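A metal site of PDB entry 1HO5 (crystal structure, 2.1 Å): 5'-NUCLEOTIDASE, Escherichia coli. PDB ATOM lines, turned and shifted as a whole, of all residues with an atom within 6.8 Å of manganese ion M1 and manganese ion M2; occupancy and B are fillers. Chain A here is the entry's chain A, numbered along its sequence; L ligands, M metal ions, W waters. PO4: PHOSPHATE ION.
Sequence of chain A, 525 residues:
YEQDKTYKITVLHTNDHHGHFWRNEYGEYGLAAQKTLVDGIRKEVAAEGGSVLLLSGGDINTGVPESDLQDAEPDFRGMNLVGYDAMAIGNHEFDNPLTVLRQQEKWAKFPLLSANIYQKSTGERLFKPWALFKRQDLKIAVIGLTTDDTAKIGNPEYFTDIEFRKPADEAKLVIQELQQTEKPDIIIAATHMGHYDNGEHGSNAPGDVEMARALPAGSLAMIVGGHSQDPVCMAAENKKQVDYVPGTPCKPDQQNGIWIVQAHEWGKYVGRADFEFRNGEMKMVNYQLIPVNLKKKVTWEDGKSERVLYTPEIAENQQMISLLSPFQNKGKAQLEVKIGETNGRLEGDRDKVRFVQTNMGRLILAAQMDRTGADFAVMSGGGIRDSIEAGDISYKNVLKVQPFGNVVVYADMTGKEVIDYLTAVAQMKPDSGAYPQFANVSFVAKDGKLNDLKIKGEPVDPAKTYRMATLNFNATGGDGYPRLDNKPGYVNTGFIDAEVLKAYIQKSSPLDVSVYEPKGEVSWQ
Manganese ion M1 is bound by OD1 of Asn 91, 2.0 Å away.
NE2 of His 192 binds manganese ion M1 (2.2 Å).
An oxygen (O4) of the ligand is bound to manganese ion M1, 2.3 Å away.
Manganese ion M1 is bound by ND1 of His 227 (2.3 Å).
Manganese ion M1 is bound by the side-chain carboxylate (OD2) of Asp 59 (2.5 Å).
Water W2 is bound to manganese ion M1 (2.6 Å).
Manganese ion M1 has six donor atoms within binding distance.
Merely in contact with manganese ion M1: His 92.
Within 4 Å of manganese ion M1: Asp 59, Asn 91, His 92, His 192 and His 227.
The nearest printed residue that does not touch manganese ion M1 is Asp 16 (4.2 Å).
Manganese ion M2 is bound by OE1 of Gln 229.
Manganese ion M2 is bound by OD2 of Asp 59, at 2.0 Å.
Manganese ion M2 is bound by the side-chain carboxylate (OD2) of Asp 16, 2.1 Å away.
Manganese ion M2 is bound by NE2 of His 18 (2.2 Å).
Water W1 binds manganese ion M2, at 2.2 Å.
Water W2 is bound to manganese ion M2 (2.3 Å).
Manganese ion M2 has six donor atoms within binding distance.
Of the 19 residues printed, 4 come within 4 Å of manganese ion M2.
The side-chain amide nitrogen (NE2) of Gln 229 lies within hydrogen-bond range of the side-chain carboxylate (OE1) of Glu 265 (2.8 Å).
The side-chain carboxylate (OD1) of Asp 59 lies within hydrogen-bond range of the backbone NH (N) of His 92.
The backbone carbonyl oxygen of Asp 59 lies within hydrogen-bond range of the backbone NH of His 17 (3.1 Å).
OD1 of Asp 16 sits at hydrogen-bond distance from N of His 227 (2.8 Å).
The backbone NH of Asp 16 is in hydrogen-bond range of the backbone carbonyl oxygen of Gly 58 (2.7 Å).
OD1 of Asp 16 sits at hydrogen-bond distance from ND2 of Asn 15 (2.7 Å).
O of His 192 sits at hydrogen-bond distance from N of Thr 147 (2.9 Å).
O of Asn 61 is in hydrogen-bond range of ND1 of His 18.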
ATOM      1  N   ASN A  15      -5.722   5.942  -8.322  1.00  0.00           N
ATOM      2  CA  ASN A  15      -7.189   5.783  -8.465  1.00  0.00           C
ATOM      3  C   ASN A  15      -7.739   5.962  -7.085  1.00  0.00           C
ATOM      4  O   ASN A  15      -6.991   5.884  -6.092  1.00  0.00           O
ATOM      5  CB  ASN A  15      -7.574   4.360  -8.897  1.00  0.00           C
ATOM      6  CG  ASN A  15      -6.934   3.335  -8.012  1.00  0.00           C
ATOM      7  OD1 ASN A  15      -5.742   3.120  -8.098  1.00  0.00           O
ATOM      8  ND2 ASN A  15      -7.697   2.753  -7.105  1.00  0.00           N
ATOM      9  N   ASP A  16      -9.047   6.189  -7.030  1.00  0.00           N
ATOM     10  CA  ASP A  16      -9.774   6.367  -5.773  1.00  0.00           C
ATOM     11  C   ASP A  16      -9.094   7.370  -4.858  1.00  0.00           C
ATOM     12  O   ASP A  16      -8.842   7.159  -3.666  1.00  0.00           O
ATOM     13  CB  ASP A  16      -9.999   5.006  -5.129  1.00  0.00           C
ATOM     14  CG  ASP A  16     -10.837   4.129  -6.026  1.00  0.00           C
ATOM     15  OD1 ASP A  16     -10.273   3.564  -6.994  1.00  0.00           O
ATOM     16  OD2 ASP A  16     -12.066   4.084  -5.814  1.00  0.00           O
ATOM     17  N   HIS A  17      -8.885   8.536  -5.447  1.00  0.00           N
ATOM     18  CA  HIS A  17      -8.221   9.609  -4.732  1.00  0.00           C
ATOM     19  C   HIS A  17      -9.059  10.050  -3.501  1.00  0.00           C
ATOM     20  O   HIS A  17      -8.507  10.272  -2.402  1.00  0.00           O
ATOM     21  CB  HIS A  17      -8.039  10.772  -5.702  1.00  0.00           C
ATOM     22  CG  HIS A  17      -7.460  11.988  -5.064  1.00  0.00           C
ATOM     23  ND1 HIS A  17      -6.137  12.060  -4.683  1.00  0.00           N
ATOM     24  CD2 HIS A  17      -8.016  13.185  -4.773  1.00  0.00           C
ATOM     25  CE1 HIS A  17      -5.891  13.276  -4.200  1.00  0.00           C
ATOM     26  NE2 HIS A  17      -7.006  13.971  -4.241  1.00  0.00           N
ATOM     27  N   HIS A  18     -10.363  10.181  -3.724  1.00  0.00           N
ATOM     28  CA  HIS A  18     -11.332  10.541  -2.703  1.00  0.00           C
ATOM     29  C   HIS A  18     -10.974  11.771  -1.839  1.00  0.00           C
ATOM     30  O   HIS A  18     -10.932  11.703  -0.604  1.00  0.00           O
ATOM     31  CB  HIS A  18     -11.623   9.303  -1.830  1.00  0.00           C
ATOM     32  CG  HIS A  18     -12.464   8.257  -2.523  1.00  0.00           C
ATOM     33  ND1 HIS A  18     -13.747   8.516  -2.979  1.00  0.00           N
ATOM     34  CD2 HIS A  18     -12.177   6.988  -2.929  1.00  0.00           C
ATOM     35  CE1 HIS A  18     -14.210   7.458  -3.631  1.00  0.00           C
ATOM     36  NE2 HIS A  18     -13.271   6.528  -3.619  1.00  0.00           N
ATOM     37  N   GLY A  58     -10.156   7.022 -11.383  1.00  0.00           N
ATOM     38  CA  GLY A  58     -11.343   7.718 -10.912  1.00  0.00           C
ATOM     39  C   GLY A  58     -11.706   7.722  -9.438  1.00  0.00           C
ATOM     40  O   GLY A  58     -10.922   7.310  -8.611  1.00  0.00           O
ATOM     41  N   ASP A  59     -12.918   8.173  -9.131  1.00  0.00           N
ATOM     42  CA  ASP A  59     -13.384   8.261  -7.733  1.00  0.00           C
ATOM     43  C   ASP A  59     -12.522   9.338  -7.019  1.00  0.00           C
ATOM     44  O   ASP A  59     -11.895   9.070  -5.973  1.00  0.00           O
ATOM     45  CB  ASP A  59     -13.228   6.883  -7.015  1.00  0.00           C
ATOM     46  CG  ASP A  59     -14.553   6.140  -6.799  1.00  0.00           C
ATOM     47  OD1 ASP A  59     -15.493   6.408  -7.536  1.00  0.00           O
ATOM     48  OD2 ASP A  59     -14.615   5.259  -5.898  1.00  0.00           O
ATOM     49  N   ASN A  61     -13.857  12.369  -6.192  1.00  0.00           N
ATOM     50  CA  ASN A  61     -14.868  12.929  -5.275  1.00  0.00           C
ATOM     51  C   ASN A  61     -15.172  12.159  -3.996  1.00  0.00           C
ATOM     52  O   ASN A  61     -15.133  10.916  -3.982  1.00  0.00           O
ATOM     53  CB  ASN A  61     -16.227  13.119  -6.026  1.00  0.00           C
ATOM     54  CG  ASN A  61     -16.211  14.280  -7.000  1.00  0.00           C
ATOM     55  OD1 ASN A  61     -16.384  15.434  -6.611  1.00  0.00           O
ATOM     56  ND2 ASN A  61     -16.009  13.987  -8.271  1.00  0.00           N
ATOM     57  N   GLY A  90     -15.369   7.799 -12.372  1.00  0.00           N
ATOM     58  CA  GLY A  90     -15.730   6.813 -11.366  1.00  0.00           C
ATOM     59  C   GLY A  90     -17.157   7.037 -10.820  1.00  0.00           C
ATOM     60  O   GLY A  90     -17.733   8.125 -10.963  1.00  0.00           O
ATOM     61  N   ASN A  91     -17.703   6.045 -10.135  1.00  0.00           N
ATOM     62  CA  ASN A  91     -19.087   6.215  -9.653  1.00  0.00           C
ATOM     63  C   ASN A  91     -19.252   7.400  -8.707  1.00  0.00           C
ATOM     64  O   ASN A  91     -20.282   8.084  -8.758  1.00  0.00           O
ATOM     65  CB  ASN A  91     -19.613   4.942  -8.994  1.00  0.00           C
ATOM     66  CG  ASN A  91     -18.725   4.445  -7.878  1.00  0.00           C
ATOM     67  OD1 ASN A  91     -17.506   4.224  -8.068  1.00  0.00           O
ATOM     68  ND2 ASN A  91     -19.321   4.226  -6.719  1.00  0.00           N
ATOM     69  N   HIS A  92     -18.273   7.640  -7.842  1.00  0.00           N
ATOM     70  CA  HIS A  92     -18.429   8.782  -6.942  1.00  0.00           C
ATOM     71  C   HIS A  92     -18.387  10.122  -7.659  1.00  0.00           C
ATOM     72  O   HIS A  92     -18.597  11.122  -7.027  1.00  0.00           O
ATOM     73  CB  HIS A  92     -17.417   8.761  -5.808  1.00  0.00           C
ATOM     74  CG  HIS A  92     -17.760   7.755  -4.775  1.00  0.00           C
ATOM     75  ND1 HIS A  92     -18.606   8.036  -3.734  1.00  0.00           N
ATOM     76  CD2 HIS A  92     -17.504   6.426  -4.711  1.00  0.00           C
ATOM     77  CE1 HIS A  92     -18.862   6.927  -3.067  1.00  0.00           C
ATOM     78  NE2 HIS A  92     -18.206   5.932  -3.649  1.00  0.00           N
ATOM     79  N   THR A 147     -17.984   1.526 -13.921  1.00  0.00           N
ATOM     80  CA  THR A 147     -18.818   0.398 -13.439  1.00  0.00           C
ATOM     81  C   THR A 147     -20.320   0.665 -13.591  1.00  0.00           C
ATOM     82  O   THR A 147     -20.798   1.768 -13.312  1.00  0.00           O
ATOM     83  CB  THR A 147     -18.563   0.084 -11.960  1.00  0.00           C
ATOM     84  OG1 THR A 147     -19.398  -1.018 -11.570  1.00  0.00           O
ATOM     85  CG2 THR A 147     -18.876   1.299 -11.051  1.00  0.00           C
ATOM     86  N   ILE A 153     -26.115   1.579  -7.110  1.00  0.00           N
ATOM     87  CA  ILE A 153     -25.800   1.869  -5.735  1.00  0.00           C
ATOM     88  C   ILE A 153     -25.805   3.367  -5.410  1.00  0.00           C
ATOM     89  O   ILE A 153     -25.655   3.761  -4.250  1.00  0.00           O
ATOM     90  CB  ILE A 153     -24.439   1.247  -5.318  1.00  0.00           C
ATOM     91  CG1 ILE A 153     -23.301   1.802  -6.158  1.00  0.00           C
ATOM     92  CG2 ILE A 153     -24.500  -0.285  -5.471  1.00  0.00           C
ATOM     93  CD1 ILE A 153     -22.020   1.042  -5.973  1.00  0.00           C
ATOM     94  N   HIS A 192     -12.981   2.189 -13.941  1.00  0.00           N
ATOM     95  CA  HIS A 192     -13.368   2.300 -12.541  1.00  0.00           C
ATOM     96  C   HIS A 192     -14.335   1.127 -12.415  1.00  0.00           C
ATOM     97  O   HIS A 192     -15.561   1.333 -12.368  1.00  0.00           O
ATOM     98  CB  HIS A 192     -14.130   3.599 -12.262  1.00  0.00           C
ATOM     99  CG  HIS A 192     -14.313   3.830 -10.794  1.00  0.00           C
ATOM    100  ND1 HIS A 192     -13.257   4.198  -9.977  1.00  0.00           N
ATOM    101  CD2 HIS A 192     -15.347   3.548  -9.980  1.00  0.00           C
ATOM    102  CE1 HIS A 192     -13.638   4.114  -8.714  1.00  0.00           C
ATOM    103  NE2 HIS A 192     -14.903   3.718  -8.686  1.00  0.00           N
ATOM    104  N   GLY A 226      -9.515   0.679 -10.702  1.00  0.00           N
ATOM    105  CA  GLY A 226      -9.891   1.333  -9.465  1.00  0.00           C
ATOM    106  C   GLY A 226     -11.157   0.704  -8.903  1.00  0.00           C
ATOM    107  O   GLY A 226     -11.439  -0.478  -9.200  1.00  0.00           O
ATOM    108  N   HIS A 227     -11.813   1.454  -8.012  1.00  0.00           N
ATOM    109  CA  HIS A 227     -13.123   1.103  -7.423  1.00  0.00           C
ATOM    110  C   HIS A 227     -13.064   0.110  -6.296  1.00  0.00           C
ATOM    111  O   HIS A 227     -13.544   0.386  -5.196  1.00  0.00           O
ATOM    112  CB  HIS A 227     -14.071   0.591  -8.580  1.00  0.00           C
ATOM    113  CG  HIS A 227     -15.500   0.342  -8.161  1.00  0.00           C
ATOM    114  ND1 HIS A 227     -16.235   1.250  -7.420  1.00  0.00           N
ATOM    115  CD2 HIS A 227     -16.340  -0.689  -8.438  1.00  0.00           C
ATOM    116  CE1 HIS A 227     -17.471   0.797  -7.269  1.00  0.00           C
ATOM    117  NE2 HIS A 227     -17.555  -0.387  -7.872  1.00  0.00           N
ATOM    118  N   SER A 228     -12.404  -1.017  -6.521  1.00  0.00           N
ATOM    119  CA  SER A 228     -12.321  -2.012  -5.485  1.00  0.00           C
ATOM    120  C   SER A 228     -11.381  -1.535  -4.413  1.00  0.00           C
ATOM    121  O   SER A 228     -11.431  -1.971  -3.253  1.00  0.00           O
ATOM    122  CB  SER A 228     -11.863  -3.364  -6.054  1.00  0.00           C
ATOM    123  OG  SER A 228     -10.713  -3.271  -6.883  1.00  0.00           O
ATOM    124  N   GLN A 229     -10.525  -0.593  -4.793  1.00  0.00           N
ATOM    125  CA  GLN A 229      -9.546  -0.028  -3.869  1.00  0.00           C
ATOM    126  C   GLN A 229      -8.589  -1.052  -3.285  1.00  0.00           C
ATOM    127  O   GLN A 229      -8.582  -1.383  -2.105  1.00  0.00           O
ATOM    128  CB  GLN A 229     -10.242   0.820  -2.795  1.00  0.00           C
ATOM    129  CG  GLN A 229     -11.058   1.980  -3.472  1.00  0.00           C
ATOM    130  CD  GLN A 229     -11.625   3.067  -2.514  1.00  0.00           C
ATOM    131  OE1 GLN A 229     -12.552   3.831  -2.883  1.00  0.00           O
ATOM    132  NE2 GLN A 229     -11.067   3.150  -1.308  1.00  0.00           N
ATOM    133  N   GLU A 265      -5.526   3.301  -3.042  1.00  0.00           N
ATOM    134  CA  GLU A 265      -6.413   4.419  -2.822  1.00  0.00           C
ATOM    135  C   GLU A 265      -5.693   5.659  -2.316  1.00  0.00           C
ATOM    136  O   GLU A 265      -4.527   5.613  -1.936  1.00  0.00           O
ATOM    137  CB  GLU A 265      -7.457   4.020  -1.759  1.00  0.00           C
ATOM    138  CG  GLU A 265      -6.825   3.794  -0.380  1.00  0.00           C
ATOM    139  CD  GLU A 265      -7.675   2.950   0.578  1.00  0.00           C
ATOM    140  OE1 GLU A 265      -8.793   2.491   0.194  1.00  0.00           O
ATOM    141  OE2 GLU A 265      -7.227   2.766   1.723  1.00  0.00           O
ATOM    142  N   ARG A 350     -16.333   0.192   7.458  1.00  0.00           N
ATOM    143  CA  ARG A 350     -17.127  -0.581   6.508  1.00  0.00           C
ATOM    144  C   ARG A 350     -17.260  -2.051   6.919  1.00  0.00           C
ATOM    145  O   ARG A 350     -18.368  -2.593   6.987  1.00  0.00           O
ATOM    146  CB  ARG A 350     -16.517  -0.475   5.102  1.00  0.00           C
ATOM    147  CG  ARG A 350     -17.534  -0.587   3.978  1.00  0.00           C
ATOM    148  CD  ARG A 350     -16.984  -1.376   2.807  1.00  0.00           C
ATOM    149  NE  ARG A 350     -16.869  -0.581   1.579  1.00  0.00           N
ATOM    150  CZ  ARG A 350     -16.654  -1.105   0.373  1.00  0.00           C
ATOM    151  NH1 ARG A 350     -16.529  -2.419   0.234  1.00  0.00           N
ATOM    152  NH2 ARG A 350     -16.552  -0.317  -0.690  1.00  0.00           N
HETATM  153  P   PO4 L   1     -17.768   2.462  -3.982  1.00  0.00           P
HETATM  154  O1  PO4 L   1     -18.420   3.295  -2.930  1.00  0.00           O
HETATM  155  O2  PO4 L   1     -16.427   1.970  -3.462  1.00  0.00           O
HETATM  156  O3  PO4 L   1     -18.628   1.287  -4.274  1.00  0.00           O
HETATM  157  O4  PO4 L   1     -17.589   3.272  -5.210  1.00  0.00           O
HETATM  158 MN    MN M   1     -16.038   3.486  -6.864  1.00  0.00          MN
HETATM  159 MN    MN M   2     -13.596   4.493  -4.381  1.00  0.00          MN
HETATM  160  O   HOH W   1     -15.374   4.556  -3.045  1.00  0.00           O
HETATM  161  O   HOH W   2     -14.702   2.522  -4.878  1.00  0.00           O
